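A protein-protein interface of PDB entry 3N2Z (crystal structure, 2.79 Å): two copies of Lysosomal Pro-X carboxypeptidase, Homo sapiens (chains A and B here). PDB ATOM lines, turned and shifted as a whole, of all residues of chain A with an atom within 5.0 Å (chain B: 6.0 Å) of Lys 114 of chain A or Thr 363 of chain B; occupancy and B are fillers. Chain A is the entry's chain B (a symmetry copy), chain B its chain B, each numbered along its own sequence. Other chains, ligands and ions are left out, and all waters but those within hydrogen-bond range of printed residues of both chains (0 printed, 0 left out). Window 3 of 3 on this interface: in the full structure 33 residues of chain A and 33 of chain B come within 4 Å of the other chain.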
ATOM      1  N   ALA A 110     -22.614  16.984 -24.664  1.00  0.00           N
ATOM      2  CA  ALA A 110     -23.859  16.294 -24.290  1.00  0.00           C
ATOM      3  C   ALA A 110     -24.502  17.040 -23.119  1.00  0.00           C
ATOM      4  O   ALA A 110     -25.679  17.381 -23.190  1.00  0.00           O
ATOM      5  CB  ALA A 110     -23.568  14.860 -23.901  1.00  0.00           C
ATOM      6  N   GLU A 111     -23.725  17.354 -22.063  1.00  0.00           N
ATOM      7  CA  GLU A 111     -24.247  18.082 -20.908  1.00  0.00           C
ATOM      8  C   GLU A 111     -24.804  19.425 -21.324  1.00  0.00           C
ATOM      9  O   GLU A 111     -25.872  19.810 -20.857  1.00  0.00           O
ATOM     10  CB  GLU A 111     -23.189  18.250 -19.817  1.00  0.00           C
ATOM     11  CG  GLU A 111     -22.597  16.937 -19.319  1.00  0.00           C
ATOM     12  CD  GLU A 111     -23.389  16.095 -18.329  1.00  0.00           C
ATOM     13  OE1 GLU A 111     -22.755  15.259 -17.643  1.00  0.00           O
ATOM     14  OE2 GLU A 111     -24.628  16.258 -18.235  1.00  0.00           O
ATOM     15  N   LEU A 112     -24.109  20.129 -22.214  1.00  0.00           N
ATOM     16  CA  LEU A 112     -24.580  21.421 -22.670  1.00  0.00           C
ATOM     17  C   LEU A 112     -25.883  21.314 -23.474  1.00  0.00           C
ATOM     18  O   LEU A 112     -26.781  22.116 -23.246  1.00  0.00           O
ATOM     19  CB  LEU A 112     -23.482  22.158 -23.440  1.00  0.00           C
ATOM     20  CG  LEU A 112     -23.834  23.546 -23.943  1.00  0.00           C
ATOM     21  CD1 LEU A 112     -24.048  24.525 -22.788  1.00  0.00           C
ATOM     22  CD2 LEU A 112     -22.811  24.033 -24.890  1.00  0.00           C
ATOM     23  N   ILE A 113     -26.003  20.332 -24.394  1.00  0.00           N
ATOM     24  CA  ILE A 113     -27.238  20.166 -25.161  1.00  0.00           C
ATOM     25  C   ILE A 113     -28.390  19.885 -24.168  1.00  0.00           C
ATOM     26  O   ILE A 113     -29.409  20.578 -24.244  1.00  0.00           O
ATOM     27  CB  ILE A 113     -27.126  19.185 -26.367  1.00  0.00           C
ATOM     28  CG1 ILE A 113     -26.059  19.685 -27.385  1.00  0.00           C
ATOM     29  CG2 ILE A 113     -28.494  19.000 -27.072  1.00  0.00           C
ATOM     30  CD1 ILE A 113     -25.777  18.757 -28.566  1.00  0.00           C
ATOM     31  N   LYS A 114     -28.186  18.954 -23.187  1.00  0.00           N
ATOM     32  CA  LYS A 114     -29.147  18.622 -22.115  1.00  0.00           C
ATOM     33  C   LYS A 114     -29.680  19.917 -21.464  1.00  0.00           C
ATOM     34  O   LYS A 114     -30.891  20.100 -21.349  1.00  0.00           O
ATOM     35  CB  LYS A 114     -28.461  17.762 -21.031  1.00  0.00           C
ATOM     36  CG  LYS A 114     -28.757  16.276 -21.097  1.00  0.00           C
ATOM     37  CD  LYS A 114     -29.447  15.776 -19.812  1.00  0.00           C
ATOM     38  CE  LYS A 114     -29.564  14.256 -19.692  1.00  0.00           C
ATOM     39  NZ  LYS A 114     -29.974  13.566 -20.961  1.00  0.00           N
ATOM     40  N   HIS A 115     -28.756  20.815 -21.073  1.00  0.00           N
ATOM     41  CA  HIS A 115     -29.023  22.111 -20.446  1.00  0.00           C
ATOM     42  C   HIS A 115     -29.852  23.046 -21.319  1.00  0.00           C
ATOM     43  O   HIS A 115     -30.756  23.690 -20.799  1.00  0.00           O
ATOM     44  CB  HIS A 115     -27.707  22.783 -20.042  1.00  0.00           C
ATOM     45  CG  HIS A 115     -27.843  24.194 -19.550  1.00  0.00           C
ATOM     46  ND1 HIS A 115     -28.298  24.476 -18.272  1.00  0.00           N
ATOM     47  CD2 HIS A 115     -27.529  25.361 -20.169  1.00  0.00           C
ATOM     48  CE1 HIS A 115     -28.271  25.797 -18.165  1.00  0.00           C
ATOM     49  NE2 HIS A 115     -27.818  26.374 -19.278  1.00  0.00           N
ATOM     50  N   LEU A 116     -29.548  23.136 -22.624  1.00  0.00           N
ATOM     51  CA  LEU A 116     -30.292  24.021 -23.520  1.00  0.00           C
ATOM     52  C   LEU A 116     -31.740  23.567 -23.694  1.00  0.00           C
ATOM     53  O   LEU A 116     -32.641  24.395 -23.653  1.00  0.00           O
ATOM     54  CB  LEU A 116     -29.595  24.177 -24.886  1.00  0.00           C
ATOM     55  CG  LEU A 116     -28.149  24.680 -24.890  1.00  0.00           C
ATOM     56  CD1 LEU A 116     -27.588  24.655 -26.275  1.00  0.00           C
ATOM     57  CD2 LEU A 116     -28.032  26.064 -24.306  1.00  0.00           C
ATOM     58  N   LYS A 117     -31.965  22.265 -23.865  1.00  0.00           N
ATOM     59  CA  LYS A 117     -33.308  21.707 -24.025  1.00  0.00           C
ATOM     60  C   LYS A 117     -34.142  21.908 -22.728  1.00  0.00           C
ATOM     61  O   LYS A 117     -35.352  22.153 -22.794  1.00  0.00           O
ATOM     62  CB  LYS A 117     -33.241  20.230 -24.446  1.00  0.00           C
ATOM     63  CG  LYS A 117     -32.516  19.991 -25.771  1.00  0.00           C
ATOM     64  CD  LYS A 117     -33.240  18.971 -26.619  1.00  0.00           C
ATOM     65  CE  LYS A 117     -32.356  18.266 -27.618  1.00  0.00           C
ATOM     66  NZ  LYS A 117     -33.151  17.581 -28.680  1.00  0.00           N
ATOM     67  N   ARG A 118     -33.471  21.858 -21.571  1.00  0.00           N
ATOM     68  CA  ARG A 118     -34.054  22.052 -20.245  1.00  0.00           C
ATOM     69  C   ARG A 118     -34.370  23.547 -20.022  1.00  0.00           C
ATOM     70  O   ARG A 118     -35.464  23.890 -19.583  1.00  0.00           O
ATOM     71  CB  ARG A 118     -33.027  21.582 -19.205  1.00  0.00           C
ATOM     72  CG  ARG A 118     -33.583  20.931 -17.950  1.00  0.00           C
ATOM     73  CD  ARG A 118     -32.455  20.328 -17.117  1.00  0.00           C
ATOM     74  NE  ARG A 118     -31.437  21.323 -16.740  1.00  0.00           N
ATOM     75  CZ  ARG A 118     -30.119  21.112 -16.753  1.00  0.00           C
ATOM     76  NH1 ARG A 118     -29.629  19.930 -17.118  1.00  0.00           N
ATOM     77  NH2 ARG A 118     -29.283  22.082 -16.399  1.00  0.00           N
ATOM     78  N   HIS A 149     -28.210   9.976 -29.648  1.00  0.00           N
ATOM     79  CA  HIS A 149     -29.378  10.438 -28.896  1.00  0.00           C
ATOM     80  C   HIS A 149     -29.330  11.947 -28.677  1.00  0.00           C
ATOM     81  O   HIS A 149     -30.343  12.503 -28.294  1.00  0.00           O
ATOM     82  CB  HIS A 149     -29.490   9.714 -27.560  1.00  0.00           C
ATOM     83  CG  HIS A 149     -28.223   9.700 -26.768  1.00  0.00           C
ATOM     84  ND1 HIS A 149     -27.266   8.705 -26.953  1.00  0.00           N
ATOM     85  CD2 HIS A 149     -27.797  10.548 -25.807  1.00  0.00           C
ATOM     86  CE1 HIS A 149     -26.300   8.974 -26.090  1.00  0.00           C
ATOM     87  NE2 HIS A 149     -26.574  10.070 -25.376  1.00  0.00           N
ATOM     88  N   MET A 150     -28.179  12.616 -28.916  1.00  0.00           N
ATOM     89  CA  MET A 150     -28.049  14.068 -28.738  1.00  0.00           C
ATOM     90  C   MET A 150     -28.160  14.810 -30.048  1.00  0.00           C
ATOM     91  O   MET A 150     -28.730  15.890 -30.079  1.00  0.00           O
ATOM     92  CB  MET A 150     -26.710  14.464 -28.081  1.00  0.00           C
ATOM     93  CG  MET A 150     -26.481  13.901 -26.691  1.00  0.00           C
ATOM     94  SD  MET A 150     -27.745  14.188 -25.415  1.00  0.00           S
ATOM     95  CE  MET A 150     -27.809  15.911 -25.363  1.00  0.00           C
ATOM     96  N   PHE B 164     -33.769   3.778 -14.768  1.00  0.00           N
ATOM     97  CA  PHE B 164     -33.150   5.026 -14.329  1.00  0.00           C
ATOM     98  C   PHE B 164     -34.088   6.181 -14.434  1.00  0.00           C
ATOM     99  O   PHE B 164     -34.978   6.178 -15.295  1.00  0.00           O
ATOM    100  CB  PHE B 164     -31.904   5.358 -15.201  1.00  0.00           C
ATOM    101  CG  PHE B 164     -30.823   4.314 -15.180  1.00  0.00           C
ATOM    102  CD1 PHE B 164     -29.833   4.337 -14.209  1.00  0.00           C
ATOM    103  CD2 PHE B 164     -30.796   3.297 -16.130  1.00  0.00           C
ATOM    104  CE1 PHE B 164     -28.832   3.360 -14.175  1.00  0.00           C
ATOM    105  CE2 PHE B 164     -29.804   2.300 -16.087  1.00  0.00           C
ATOM    106  CZ  PHE B 164     -28.830   2.342 -15.108  1.00  0.00           C
ATOM    107  N   GLU B 165     -33.852   7.202 -13.575  1.00  0.00           N
ATOM    108  CA  GLU B 165     -34.603   8.438 -13.534  1.00  0.00           C
ATOM    109  C   GLU B 165     -36.107   8.213 -13.606  1.00  0.00           C
ATOM    110  O   GLU B 165     -36.659   7.408 -12.847  1.00  0.00           O
ATOM    111  CB  GLU B 165     -34.136   9.365 -14.658  1.00  0.00           C
ATOM    112  CG  GLU B 165     -32.660   9.694 -14.594  1.00  0.00           C
ATOM    113  CD  GLU B 165     -32.318  10.946 -15.370  1.00  0.00           C
ATOM    114  OE1 GLU B 165     -32.229  12.030 -14.744  1.00  0.00           O
ATOM    115  OE2 GLU B 165     -32.160  10.848 -16.607  1.00  0.00           O
ATOM    116  N   LEU B 167     -37.553   7.190 -16.520  1.00  0.00           N
ATOM    117  CA  LEU B 167     -37.786   6.325 -17.679  1.00  0.00           C
ATOM    118  C   LEU B 167     -38.920   5.332 -17.466  1.00  0.00           C
ATOM    119  O   LEU B 167     -39.765   5.158 -18.359  1.00  0.00           O
ATOM    120  CB  LEU B 167     -36.496   5.630 -18.161  1.00  0.00           C
ATOM    121  CG  LEU B 167     -35.367   6.541 -18.672  1.00  0.00           C
ATOM    122  CD1 LEU B 167     -34.220   5.722 -19.200  1.00  0.00           C
ATOM    123  CD2 LEU B 167     -35.856   7.505 -19.724  1.00  0.00           C
ATOM    124  N   PRO B 359     -27.222  10.871 -10.732  1.00  0.00           N
ATOM    125  CA  PRO B 359     -28.418  10.130 -11.184  1.00  0.00           C
ATOM    126  C   PRO B 359     -28.835  10.258 -12.639  1.00  0.00           C
ATOM    127  O   PRO B 359     -29.704   9.497 -13.068  1.00  0.00           O
ATOM    128  CB  PRO B 359     -29.512  10.664 -10.246  1.00  0.00           C
ATOM    129  CG  PRO B 359     -29.075  12.056  -9.943  1.00  0.00           C
ATOM    130  CD  PRO B 359     -27.599  11.870  -9.708  1.00  0.00           C
ATOM    131  N   SER B 360     -28.246  11.215 -13.385  1.00  0.00           N
ATOM    132  CA  SER B 360     -28.595  11.461 -14.789  1.00  0.00           C
ATOM    133  C   SER B 360     -27.530  10.998 -15.774  1.00  0.00           C
ATOM    134  O   SER B 360     -27.774  10.983 -16.984  1.00  0.00           O
ATOM    135  CB  SER B 360     -28.906  12.937 -15.008  1.00  0.00           C
ATOM    136  OG  SER B 360     -27.805  13.588 -15.625  1.00  0.00           O
ATOM    137  N   TRP B 361     -26.359  10.640 -15.258  1.00  0.00           N
ATOM    138  CA  TRP B 361     -25.230  10.231 -16.070  1.00  0.00           C
ATOM    139  C   TRP B 361     -25.457   9.147 -17.125  1.00  0.00           C
ATOM    140  O   TRP B 361     -25.269   9.434 -18.303  1.00  0.00           O
ATOM    141  CB  TRP B 361     -23.964  10.010 -15.236  1.00  0.00           C
ATOM    142  CG  TRP B 361     -22.767   9.641 -16.072  1.00  0.00           C
ATOM    143  CD1 TRP B 361     -22.044   8.484 -15.994  1.00  0.00           C
ATOM    144  CD2 TRP B 361     -22.167  10.421 -17.119  1.00  0.00           C
ATOM    145  NE1 TRP B 361     -21.032   8.494 -16.924  1.00  0.00           N
ATOM    146  CE2 TRP B 361     -21.070   9.680 -17.617  1.00  0.00           C
ATOM    147  CE3 TRP B 361     -22.454  11.671 -17.695  1.00  0.00           C
ATOM    148  CZ2 TRP B 361     -20.255  10.151 -18.656  1.00  0.00           C
ATOM    149  CZ3 TRP B 361     -21.657  12.131 -18.740  1.00  0.00           C
ATOM    150  CH2 TRP B 361     -20.563  11.383 -19.196  1.00  0.00           C
ATOM    151  N   ILE B 362     -25.848   7.923 -16.713  1.00  0.00           N
ATOM    152  CA  ILE B 362     -26.101   6.763 -17.577  1.00  0.00           C
ATOM    153  C   ILE B 362     -26.986   7.116 -18.772  1.00  0.00           C
ATOM    154  O   ILE B 362     -26.771   6.627 -19.875  1.00  0.00           O
ATOM    155  CB  ILE B 362     -26.637   5.568 -16.740  1.00  0.00           C
ATOM    156  CG1 ILE B 362     -25.557   5.022 -15.780  1.00  0.00           C
ATOM    157  CG2 ILE B 362     -27.244   4.453 -17.603  1.00  0.00           C
ATOM    158  CD1 ILE B 362     -24.331   4.297 -16.376  1.00  0.00           C
ATOM    159  N   THR B 363     -27.936   7.982 -18.548  1.00  0.00           N
ATOM    160  CA  THR B 363     -28.892   8.481 -19.513  1.00  0.00           C
ATOM    161  C   THR B 363     -28.248   9.425 -20.524  1.00  0.00           C
ATOM    162  O   THR B 363     -28.651   9.444 -21.695  1.00  0.00           O
ATOM    163  CB  THR B 363     -30.010   9.074 -18.709  1.00  0.00           C
ATOM    164  OG1 THR B 363     -31.030   8.089 -18.606  1.00  0.00           O
ATOM    165  CG2 THR B 363     -30.480  10.417 -19.207  1.00  0.00           C
ATOM    166  N   THR B 364     -27.259  10.216 -20.072  1.00  0.00           N
ATOM    167  CA  THR B 364     -26.536  11.150 -20.928  1.00  0.00           C
ATOM    168  C   THR B 364     -25.536  10.358 -21.763  1.00  0.00           C
ATOM    169  O   THR B 364     -25.376  10.648 -22.947  1.00  0.00           O
ATOM    170  CB  THR B 364     -25.852  12.222 -20.086  1.00  0.00           C
ATOM    171  OG1 THR B 364     -26.818  12.815 -19.227  1.00  0.00           O
ATOM    172  CG2 THR B 364     -25.208  13.300 -20.924  1.00  0.00           C
ATOM    173  N   MET B 365     -24.875   9.359 -21.155  1.00  0.00           N
ATOM    174  CA  MET B 365     -23.881   8.546 -21.830  1.00  0.00           C
ATOM    175  C   MET B 365     -24.518   7.547 -22.842  1.00  0.00           C
ATOM    176  O   MET B 365     -24.293   7.658 -24.051  1.00  0.00           O
ATOM    177  CB  MET B 365     -22.995   7.838 -20.784  1.00  0.00           C
ATOM    178  CG  MET B 365     -21.904   6.951 -21.371  1.00  0.00           C
ATOM    179  SD  MET B 365     -20.620   7.902 -22.214  1.00  0.00           S
ATOM    180  CE  MET B 365     -19.504   6.594 -22.659  1.00  0.00           C
ATOM    181  N   TYR B 366     -25.315   6.592 -22.328  1.00  0.00           N
ATOM    182  CA  TYR B 366     -25.952   5.535 -23.089  1.00  0.00           C
ATOM    183  C   TYR B 366     -27.310   5.801 -23.799  1.00  0.00           C
ATOM    184  O   TYR B 366     -27.825   4.910 -24.477  1.00  0.00           O
ATOM    185  CB  TYR B 366     -25.901   4.246 -22.302  1.00  0.00           C
ATOM    186  CG  TYR B 366     -24.525   3.946 -21.744  1.00  0.00           C
ATOM    187  CD1 TYR B 366     -23.481   3.542 -22.577  1.00  0.00           C
ATOM    188  CD2 TYR B 366     -24.269   4.044 -20.380  1.00  0.00           C
ATOM    189  CE1 TYR B 366     -22.217   3.256 -22.065  1.00  0.00           C
ATOM    190  CE2 TYR B 366     -23.014   3.744 -19.855  1.00  0.00           C
ATOM    191  CZ  TYR B 366     -21.985   3.366 -20.702  1.00  0.00           C
ATOM    192  OH  TYR B 366     -20.749   3.077 -20.166  1.00  0.00           O
ATOM    193  N   GLY B 367     -27.847   7.014 -23.664  1.00  0.00           N
ATOM    194  CA  GLY B 367     -29.030   7.474 -24.389  1.00  0.00           C
ATOM    195  C   GLY B 367     -30.436   7.330 -23.873  1.00  0.00           C
ATOM    196  O   GLY B 367     -31.349   7.980 -24.420  1.00  0.00           O
ATOM    197  N   GLY B 368     -30.605   6.478 -22.851  1.00  0.00           N
ATOM    198  CA  GLY B 368     -31.904   6.206 -22.263  1.00  0.00           C
ATOM    199  C   GLY B 368     -32.769   5.439 -23.233  1.00  0.00           C
ATOM    200  O   GLY B 368     -32.358   4.402 -23.768  1.00  0.00           O
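Ala 110 of chain A touches Thr 364 of chain B. Glu 111 of chain A touches Trp 361 of chain B (OE1 to CZ3, 3.5 Å). Lys 114 of chain A touches Thr 363 of chain B (NZ to CG2, 3.6 Å). OG1 of Thr 364 of chain B touches CE of Lys 114 of chain A (3.1 Å). His 149 of chain A touches Met 365 of chain B (CE1 to O, 3.1 Å). His 149 of chain A touches Gly 367 of chain B.
Among the printed residues, 7 pairs touch across the chains. Among the printed residues, no Asp or Glu carboxylate lies within 4 Å of a Lys or Arg side-chain nitrogen of the other chain.
O of Thr 364 of chain B is in hydrogen-bond range of NE2 of His 149 of chain A.
Of chain B, only Thr 363 and Thr 364 come within 4 Å of Lys 114 of chain A. Of the printed residues of chain A, Thr 363 of chain B touches Lys 114 (3.6 Å). Printed residues of chain A within 4 Å of Met 365 of chain B: His 149. Printed residues of chain B within 4 Å of Ala 110 of chain A: Thr 364 (3.7 Å). Printed residues of chain A within 4 Å of Gly 367 of chain B: His 149 (3.3 Å). Of the printed residues of chain B, Glu 111 of chain A touches Trp 361. Printed residues of chain A within 4 Å of Thr 364 of chain B: Ala 110, Lys 114 and His 149. His 115 of chain A touches none of the printed residues of chain B. The nearest printed residue of chain B that does not touch Ala 110 of chain A is Trp 361 of chain B (6.1 Å).
The side-chain hydroxyl (OG1) of Thr 364 of chain B sits at hydrogen-bond distance from the backbone carbonyl oxygen (O) of Ser 360 of chain B (3.0 Å).
No position is printed for both chains. Of the 7 pairs that touch across the chains among the printed residues, none has its exchanged pair printed and touching as well.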
